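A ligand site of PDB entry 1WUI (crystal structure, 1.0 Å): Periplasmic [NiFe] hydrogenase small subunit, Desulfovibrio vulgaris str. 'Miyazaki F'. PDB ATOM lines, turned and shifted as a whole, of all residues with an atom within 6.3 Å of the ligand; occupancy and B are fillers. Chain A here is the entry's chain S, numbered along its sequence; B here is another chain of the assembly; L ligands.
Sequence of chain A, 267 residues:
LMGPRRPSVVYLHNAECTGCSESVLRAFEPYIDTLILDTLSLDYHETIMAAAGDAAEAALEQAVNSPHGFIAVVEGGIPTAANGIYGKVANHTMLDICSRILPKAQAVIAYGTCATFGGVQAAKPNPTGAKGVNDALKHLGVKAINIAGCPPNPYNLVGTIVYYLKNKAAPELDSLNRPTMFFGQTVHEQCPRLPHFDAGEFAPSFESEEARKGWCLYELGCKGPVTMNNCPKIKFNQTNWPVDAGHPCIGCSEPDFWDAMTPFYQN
SG of Cys 114 is bound to FE2 of the ligand, 2.3 Å away. The backbone NH (N) of Cys 17 sits close to a sulfur (S3) of the ligand, 3.5 Å away. N of Cys 114 lies close to S1 of the ligand, 3.5 Å away. ND1 of His 217 of chain B sits close to S2 of the ligand (3.7 Å). The backbone NH (N) of Thr 113 sits close to a sulfur (S1) of the ligand (3.4 Å). The side-chain sulfur (SG) of Cys 20 binds an iron atom (FE4) of the ligand (2.2 Å). SG of Cys 17 binds FE1 of the ligand (2.3 Å). An iron atom (FE3) of the ligand is bound by the side-chain sulfur of Cys 150 (2.3 Å).
O of Tyr 111 sits close to SG of Cys 20, 3.8 Å away. The side-chain sulfur (SG) of Cys 114 lies close to the side-chain amide nitrogen (NE2) of Gln 121 (3.3 Å). O of Cys 150 lies within hydrogen-bond range of ND1 of His 217 of chain B. The guanidinium group (NH1) of Arg 41 of chain B lies within hydrogen-bond range of the backbone carbonyl oxygen (O) of Arg 61 of chain B (2.8 Å). A ring nitrogen (ND1) of His 217 of chain B is in hydrogen-bond range of the guanidinium group of Arg 61 of chain B (3.5 Å). The backbone carbonyl oxygen of Cys 17 lies within hydrogen-bond range of the backbone NH of Gly 64 of chain B, at 2.8 Å. SG of Cys 114 sits close to N of Val 120 (3.8 Å). OE1 of Glu 75 is in hydrogen-bond range of N of Cys 20, at 3.1 Å.
The backbone carbonyl oxygen (O) of Gly 149 sits close to a sulfur (S1) of the ligand (3.6 Å). The backbone nitrogen (N) of Pro 151 sits close to a sulfur (S2) of the ligand (3.6 Å). Glu 16 touches the ligand. Gly 19 touches the ligand (CA to S2, 3.9 Å). OE1 of Glu 75 touches S3 of the ligand, 3.9 Å away. Gly 112 touches the ligand (C to S1, 3.8 Å). CG of Arg 61 of chain B touches S4 of the ligand, at 3.4 Å. Hydrophobic or aromatic side chains within 4 Å of the ligand: Pro 151 and His 217 of chain B. 13 residues have an atom within 4 Å of the ligand: Glu 16, Cys 17, Gly 19, Cys 20, Glu 75, Gly 112, Thr 113, Cys 114, Gly 149, Cys 150, Pro 151, Arg 61 of chain B and His 217 of chain B.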
ATOM      1  N   ALA A  15      16.798  -5.176 -28.050  1.00  0.00           N
ATOM      2  CA  ALA A  15      15.661  -4.253 -28.053  1.00  0.00           C
ATOM      3  C   ALA A  15      14.606  -4.912 -27.190  1.00  0.00           C
ATOM      4  O   ALA A  15      13.898  -5.827 -27.595  1.00  0.00           O
ATOM      5  CB  ALA A  15      15.185  -4.003 -29.472  1.00  0.00           C
ATOM      6  N   GLU A  16      14.514  -4.399 -25.953  1.00  0.00           N
ATOM      7  CA  GLU A  16      13.755  -5.058 -24.905  1.00  0.00           C
ATOM      8  C   GLU A  16      13.273  -4.001 -23.910  1.00  0.00           C
ATOM      9  O   GLU A  16      13.719  -2.880 -23.911  1.00  0.00           O
ATOM     10  CB  GLU A  16      14.598  -6.162 -24.221  1.00  0.00           C
ATOM     11  CG  GLU A  16      15.995  -5.755 -23.838  1.00  0.00           C
ATOM     12  CD  GLU A  16      16.184  -4.923 -22.605  1.00  0.00           C
ATOM     13  OE1 GLU A  16      15.496  -5.245 -21.632  1.00  0.00           O
ATOM     14  OE2 GLU A  16      17.062  -4.065 -22.616  1.00  0.00           O
ATOM     15  N   CYS A  17      12.318  -4.438 -23.074  1.00  0.00           N
ATOM     16  CA  CYS A  17      11.694  -3.572 -22.070  1.00  0.00           C
ATOM     17  C   CYS A  17      12.154  -3.966 -20.676  1.00  0.00           C
ATOM     18  O   CYS A  17      11.735  -3.310 -19.710  1.00  0.00           O
ATOM     19  CB  CYS A  17      10.154  -3.659 -22.161  1.00  0.00           C
ATOM     20  SG  CYS A  17       9.409  -5.090 -21.362  1.00  0.00           S
ATOM     21  N   THR A  18      12.926  -5.025 -20.531  1.00  0.00           N
ATOM     22  CA  THR A  18      13.478  -5.530 -19.258  1.00  0.00           C
ATOM     23  C   THR A  18      12.427  -6.278 -18.494  1.00  0.00           C
ATOM     24  O   THR A  18      12.703  -6.813 -17.399  1.00  0.00           O
ATOM     25  CB  THR A  18      14.227  -4.434 -18.462  1.00  0.00           C
ATOM     26  OG1 THR A  18      15.094  -3.755 -19.406  1.00  0.00           O
ATOM     27  CG2 THR A  18      15.073  -4.977 -17.349  1.00  0.00           C
ATOM     28  N   GLY A  19      11.226  -6.433 -19.040  1.00  0.00           N
ATOM     29  CA  GLY A  19      10.189  -7.269 -18.416  1.00  0.00           C
ATOM     30  C   GLY A  19      10.596  -8.714 -18.346  1.00  0.00           C
ATOM     31  O   GLY A  19      10.221  -9.433 -17.399  1.00  0.00           O
ATOM     32  N   CYS A  20      11.328  -9.212 -19.341  1.00  0.00           N
ATOM     33  CA  CYS A  20      11.819 -10.585 -19.252  1.00  0.00           C
ATOM     34  C   CYS A  20      12.829 -10.749 -18.148  1.00  0.00           C
ATOM     35  O   CYS A  20      12.763 -11.707 -17.372  1.00  0.00           O
ATOM     36  CB  CYS A  20      12.335 -11.027 -20.647  1.00  0.00           C
ATOM     37  SG  CYS A  20      10.984 -11.322 -21.842  1.00  0.00           S
ATOM     38  N   SER A  21      13.760  -9.799 -18.008  1.00  0.00           N
ATOM     39  CA  SER A  21      14.679  -9.874 -16.877  1.00  0.00           C
ATOM     40  C   SER A  21      13.910  -9.887 -15.542  1.00  0.00           C
ATOM     41  O   SER A  21      14.256 -10.636 -14.638  1.00  0.00           O
ATOM     42  CB  SER A  21      15.624  -8.667 -16.861  1.00  0.00           C
ATOM     43  OG  SER A  21      16.678  -8.802 -17.805  1.00  0.00           O
ATOM     44  N   GLU A  75      17.517 -11.588 -24.299  1.00  0.00           N
ATOM     45  CA  GLU A  75      16.301 -10.845 -24.140  1.00  0.00           C
ATOM     46  C   GLU A  75      16.257  -9.716 -25.182  1.00  0.00           C
ATOM     47  O   GLU A  75      17.238  -8.995 -25.326  1.00  0.00           O
ATOM     48  CB  GLU A  75      16.251 -10.238 -22.722  1.00  0.00           C
ATOM     49  CG  GLU A  75      15.031  -9.356 -22.429  1.00  0.00           C
ATOM     50  CD  GLU A  75      14.940  -8.933 -20.970  1.00  0.00           C
ATOM     51  OE1 GLU A  75      13.975  -8.255 -20.563  1.00  0.00           O
ATOM     52  OE2 GLU A  75      15.891  -9.326 -20.232  1.00  0.00           O
ATOM     53  N   GLY A  76      15.144  -9.615 -25.911  1.00  0.00           N
ATOM     54  CA  GLY A  76      14.938  -8.546 -26.881  1.00  0.00           C
ATOM     55  C   GLY A  76      15.208  -8.982 -28.309  1.00  0.00           C
ATOM     56  O   GLY A  76      15.957  -9.854 -28.608  1.00  0.00           O
ATOM     57  N   GLY A  77      14.510  -8.275 -29.192  1.00  0.00           N
ATOM     58  CA  GLY A  77      14.696  -8.413 -30.641  1.00  0.00           C
ATOM     59  C   GLY A  77      15.963  -7.712 -31.084  1.00  0.00           C
ATOM     60  O   GLY A  77      16.487  -6.816 -30.403  1.00  0.00           O
ATOM     61  N   TYR A 111      14.802 -15.697 -24.815  1.00  0.00           N
ATOM     62  CA  TYR A 111      13.821 -15.608 -23.714  1.00  0.00           C
ATOM     63  C   TYR A 111      12.954 -14.380 -23.954  1.00  0.00           C
ATOM     64  O   TYR A 111      13.425 -13.249 -23.943  1.00  0.00           O
ATOM     65  CB  TYR A 111      14.582 -15.552 -22.391  1.00  0.00           C
ATOM     66  CG  TYR A 111      13.633 -15.575 -21.191  1.00  0.00           C
ATOM     67  CD1 TYR A 111      12.795 -16.665 -20.982  1.00  0.00           C
ATOM     68  CD2 TYR A 111      13.598 -14.527 -20.290  1.00  0.00           C
ATOM     69  CE1 TYR A 111      11.946 -16.725 -19.914  1.00  0.00           C
ATOM     70  CE2 TYR A 111      12.705 -14.589 -19.234  1.00  0.00           C
ATOM     71  CZ  TYR A 111      11.861 -15.666 -19.034  1.00  0.00           C
ATOM     72  OH  TYR A 111      10.994 -15.770 -17.991  1.00  0.00           O
ATOM     73  N   GLY A 112      11.660 -14.652 -24.161  1.00  0.00           N
ATOM     74  CA  GLY A 112      10.620 -13.689 -24.400  1.00  0.00           C
ATOM     75  C   GLY A 112      10.299 -13.583 -25.881  1.00  0.00           C
ATOM     76  O   GLY A 112      11.175 -13.763 -26.741  1.00  0.00           O
ATOM     77  N   THR A 113       9.065 -13.252 -26.177  1.00  0.00           N
ATOM     78  CA  THR A 113       8.582 -13.101 -27.556  1.00  0.00           C
ATOM     79  C   THR A 113       9.418 -12.160 -28.383  1.00  0.00           C
ATOM     80  O   THR A 113       9.558 -12.370 -29.589  1.00  0.00           O
ATOM     81  CB  THR A 113       7.106 -12.696 -27.505  1.00  0.00           C
ATOM     82  OG1 THR A 113       6.454 -13.858 -26.939  1.00  0.00           O
ATOM     83  CG2 THR A 113       6.535 -12.390 -28.880  1.00  0.00           C
ATOM     84  N   CYS A 114       9.972 -11.101 -27.815  1.00  0.00           N
ATOM     85  CA  CYS A 114      10.878 -10.258 -28.611  1.00  0.00           C
ATOM     86  C   CYS A 114      12.098 -11.019 -29.123  1.00  0.00           C
ATOM     87  O   CYS A 114      12.399 -10.969 -30.330  1.00  0.00           O
ATOM     88  CB  CYS A 114      11.382  -9.072 -27.820  1.00  0.00           C
ATOM     89  SG  CYS A 114      10.067  -7.880 -27.326  1.00  0.00           S
ATOM     90  N   ALA A 115      12.809 -11.721 -28.230  1.00  0.00           N
ATOM     91  CA  ALA A 115      13.975 -12.487 -28.683  1.00  0.00           C
ATOM     92  C   ALA A 115      13.542 -13.650 -29.551  1.00  0.00           C
ATOM     93  O   ALA A 115      14.283 -14.051 -30.476  1.00  0.00           O
ATOM     94  CB  ALA A 115      14.762 -12.992 -27.496  1.00  0.00           C
ATOM     95  N   GLY A 119       8.800  -9.516 -31.521  1.00  0.00           N
ATOM     96  CA  GLY A 119       8.071  -8.831 -30.467  1.00  0.00           C
ATOM     97  C   GLY A 119       7.586  -7.455 -30.806  1.00  0.00           C
ATOM     98  O   GLY A 119       7.327  -7.085 -31.948  1.00  0.00           O
ATOM     99  N   VAL A 120       7.447  -6.619 -29.758  1.00  0.00           N
ATOM    100  CA  VAL A 120       6.646  -5.421 -29.869  1.00  0.00           C
ATOM    101  C   VAL A 120       7.255  -4.443 -30.887  1.00  0.00           C
ATOM    102  O   VAL A 120       6.539  -3.816 -31.658  1.00  0.00           O
ATOM    103  CB  VAL A 120       6.406  -4.777 -28.480  1.00  0.00           C
ATOM    104  CG1 VAL A 120       7.665  -4.220 -27.853  1.00  0.00           C
ATOM    105  CG2 VAL A 120       5.317  -3.732 -28.581  1.00  0.00           C
ATOM    106  N   GLN A 121       8.566  -4.273 -30.901  1.00  0.00           N
ATOM    107  CA  GLN A 121       9.204  -3.359 -31.835  1.00  0.00           C
ATOM    108  C   GLN A 121       9.173  -3.898 -33.267  1.00  0.00           C
ATOM    109  O   GLN A 121       9.391  -3.116 -34.200  1.00  0.00           O
ATOM    110  CB  GLN A 121      10.632  -3.011 -31.427  1.00  0.00           C
ATOM    111  CG  GLN A 121      11.604  -4.192 -31.221  1.00  0.00           C
ATOM    112  CD  GLN A 121      11.487  -4.781 -29.845  1.00  0.00           C
ATOM    113  OE1 GLN A 121      11.473  -4.034 -28.855  1.00  0.00           O
ATOM    114  NE2 GLN A 121      11.395  -6.103 -29.730  1.00  0.00           N
ATOM    115  N   GLY A 149       6.528 -15.677 -24.751  1.00  0.00           N
ATOM    116  CA  GLY A 149       5.668 -15.012 -23.811  1.00  0.00           C
ATOM    117  C   GLY A 149       6.212 -13.587 -23.588  1.00  0.00           C
ATOM    118  O   GLY A 149       7.367 -13.307 -23.824  1.00  0.00           O
ATOM    119  N   CYS A 150       5.320 -12.735 -23.052  1.00  0.00           N
ATOM    120  CA  CYS A 150       5.606 -11.297 -22.972  1.00  0.00           C
ATOM    121  C   CYS A 150       5.260 -10.727 -21.592  1.00  0.00           C
ATOM    122  O   CYS A 150       4.353  -9.913 -21.462  1.00  0.00           O
ATOM    123  CB  CYS A 150       4.918 -10.575 -24.135  1.00  0.00           C
ATOM    124  SG  CYS A 150       5.490  -8.886 -24.447  1.00  0.00           S
ATOM    125  N   PRO A 151       6.028 -11.109 -20.574  1.00  0.00           N
ATOM    126  CA  PRO A 151       7.143 -12.031 -20.592  1.00  0.00           C
ATOM    127  C   PRO A 151       6.707 -13.459 -20.401  1.00  0.00           C
ATOM    128  O   PRO A 151       5.577 -13.765 -20.006  1.00  0.00           O
ATOM    129  CB  PRO A 151       7.980 -11.566 -19.427  1.00  0.00           C
ATOM    130  CG  PRO A 151       6.958 -11.090 -18.438  1.00  0.00           C
ATOM    131  CD  PRO A 151       5.858 -10.475 -19.246  1.00  0.00           C
ATOM    132  N   PRO A 152       7.596 -14.414 -20.666  1.00  0.00           N
ATOM    133  CA  PRO A 152       7.306 -15.834 -20.393  1.00  0.00           C
ATOM    134  C   PRO A 152       7.150 -16.049 -18.909  1.00  0.00           C
ATOM    135  O   PRO A 152       7.552 -15.253 -18.048  1.00  0.00           O
ATOM    136  CB  PRO A 152       8.563 -16.559 -20.880  1.00  0.00           C
ATOM    137  CG  PRO A 152       9.261 -15.556 -21.754  1.00  0.00           C
ATOM    138  CD  PRO A 152       8.980 -14.247 -21.132  1.00  0.00           C
ATOM    139  N   TRP A 258       1.268  -9.124 -31.991  1.00  0.00           N
ATOM    140  CA  TRP A 258       0.849  -7.713 -31.994  1.00  0.00           C
ATOM    141  C   TRP A 258      -0.007  -7.370 -33.238  1.00  0.00           C
ATOM    142  O   TRP A 258      -0.881  -6.551 -33.168  1.00  0.00           O
ATOM    143  CB  TRP A 258       2.096  -6.826 -31.967  1.00  0.00           C
ATOM    144  CG  TRP A 258       2.868  -7.032 -30.680  1.00  0.00           C
ATOM    145  CD1 TRP A 258       4.027  -7.748 -30.565  1.00  0.00           C
ATOM    146  CD2 TRP A 258       2.524  -6.584 -29.383  1.00  0.00           C
ATOM    147  NE1 TRP A 258       4.423  -7.742 -29.202  1.00  0.00           N
ATOM    148  CE2 TRP A 258       3.504  -7.049 -28.501  1.00  0.00           C
ATOM    149  CE3 TRP A 258       1.446  -5.870 -28.883  1.00  0.00           C
ATOM    150  CZ2 TRP A 258       3.458  -6.776 -27.117  1.00  0.00           C
ATOM    151  CZ3 TRP A 258       1.406  -5.608 -27.530  1.00  0.00           C
ATOM    152  CH2 TRP A 258       2.377  -6.065 -26.678  1.00  0.00           C
ATOM    153  N   ARG B  41      12.994   2.018 -30.229  1.00  0.00           N
ATOM    154  CA  ARG B  41      12.024   1.019 -30.676  1.00  0.00           C
ATOM    155  C   ARG B  41      10.907   1.622 -31.525  1.00  0.00           C
ATOM    156  O   ARG B  41      10.460   0.985 -32.481  1.00  0.00           O
ATOM    157  CB  ARG B  41      11.446   0.237 -29.487  1.00  0.00           C
ATOM    158  CG  ARG B  41      12.457  -0.691 -28.853  1.00  0.00           C
ATOM    159  CD  ARG B  41      12.033  -1.394 -27.563  1.00  0.00           C
ATOM    160  NE  ARG B  41      11.777  -0.365 -26.558  1.00  0.00           N
ATOM    161  CZ  ARG B  41      10.892  -0.455 -25.574  1.00  0.00           C
ATOM    162  NH1 ARG B  41      10.220  -1.564 -25.325  1.00  0.00           N
ATOM    163  NH2 ARG B  41      10.692   0.620 -24.815  1.00  0.00           N
ATOM    164  N   ARG B  61       4.497  -2.447 -22.752  1.00  0.00           N
ATOM    165  CA  ARG B  61       5.804  -2.950 -23.166  1.00  0.00           C
ATOM    166  C   ARG B  61       6.829  -1.873 -23.454  1.00  0.00           C
ATOM    167  O   ARG B  61       7.951  -2.195 -23.833  1.00  0.00           O
ATOM    168  CB  ARG B  61       5.665  -3.931 -24.324  1.00  0.00           C
ATOM    169  CG  ARG B  61       5.167  -5.307 -23.968  1.00  0.00           C
ATOM    170  CD  ARG B  61       3.779  -5.335 -23.367  1.00  0.00           C
ATOM    171  NE  ARG B  61       3.380  -6.727 -23.142  1.00  0.00           N
ATOM    172  CZ  ARG B  61       2.252  -7.092 -22.613  1.00  0.00           C
ATOM    173  NH1 ARG B  61       1.279  -6.178 -22.443  1.00  0.00           N
ATOM    174  NH2 ARG B  61       2.113  -8.334 -22.248  1.00  0.00           N
ATOM    175  N   GLY B  64       9.229  -2.965 -18.515  1.00  0.00           N
ATOM    176  CA  GLY B  64       8.847  -4.017 -17.582  1.00  0.00           C
ATOM    177  C   GLY B  64       9.395  -3.826 -16.187  1.00  0.00           C
ATOM    178  O   GLY B  64       9.055  -4.638 -15.320  1.00  0.00           O
ATOM    179  N   PRO B 216       5.681  -9.728 -14.307  1.00  0.00           N
ATOM    180  CA  PRO B 216       5.444  -8.460 -14.996  1.00  0.00           C
ATOM    181  C   PRO B 216       4.281  -8.518 -15.973  1.00  0.00           C
ATOM    182  O   PRO B 216       3.841  -9.511 -16.482  1.00  0.00           O
ATOM    183  CB  PRO B 216       6.746  -8.183 -15.763  1.00  0.00           C
ATOM    184  CG  PRO B 216       7.776  -9.041 -15.052  1.00  0.00           C
ATOM    185  CD  PRO B 216       6.990 -10.281 -14.666  1.00  0.00           C
ATOM    186  N   HIS B 217       3.797  -7.353 -16.274  1.00  0.00           N
ATOM    187  CA  HIS B 217       2.860  -6.880 -17.305  1.00  0.00           C
ATOM    188  C   HIS B 217       1.477  -7.332 -16.908  1.00  0.00           C
ATOM    189  O   HIS B 217       0.990  -8.396 -17.285  1.00  0.00           O
ATOM    190  CB  HIS B 217       3.286  -7.306 -18.709  1.00  0.00           C
ATOM    191  CG  HIS B 217       4.486  -6.528 -19.206  1.00  0.00           C
ATOM    192  ND1 HIS B 217       5.307  -6.831 -20.230  1.00  0.00           N
ATOM    193  CD2 HIS B 217       4.872  -5.299 -18.674  1.00  0.00           C
ATOM    194  CE1 HIS B 217       6.210  -5.800 -20.334  1.00  0.00           C
ATOM    195  NE2 HIS B 217       5.915  -4.888 -19.401  1.00  0.00           N
HETATM  196 FE1  LIG L   1       9.420  -6.853 -22.787  1.00  0.00          FE
HETATM  197 FE2  LIG L   1       9.880  -8.142 -25.083  1.00  0.00          FE
HETATM  198 FE3  LIG L   1       7.639  -8.615 -23.746  1.00  0.00          FE
HETATM  199 FE4  LIG L   1      10.024  -9.510 -22.707  1.00  0.00          FE
HETATM  200  S1  LIG L   1       9.026 -10.244 -24.605  1.00  0.00           S
HETATM  201  S2  LIG L   1       8.281  -8.480 -21.592  1.00  0.00           S
HETATM  202  S3  LIG L   1      11.417  -7.816 -23.470  1.00  0.00           S
HETATM  203  S4  LIG L   1       8.273  -6.572 -24.665  1.00  0.00           S
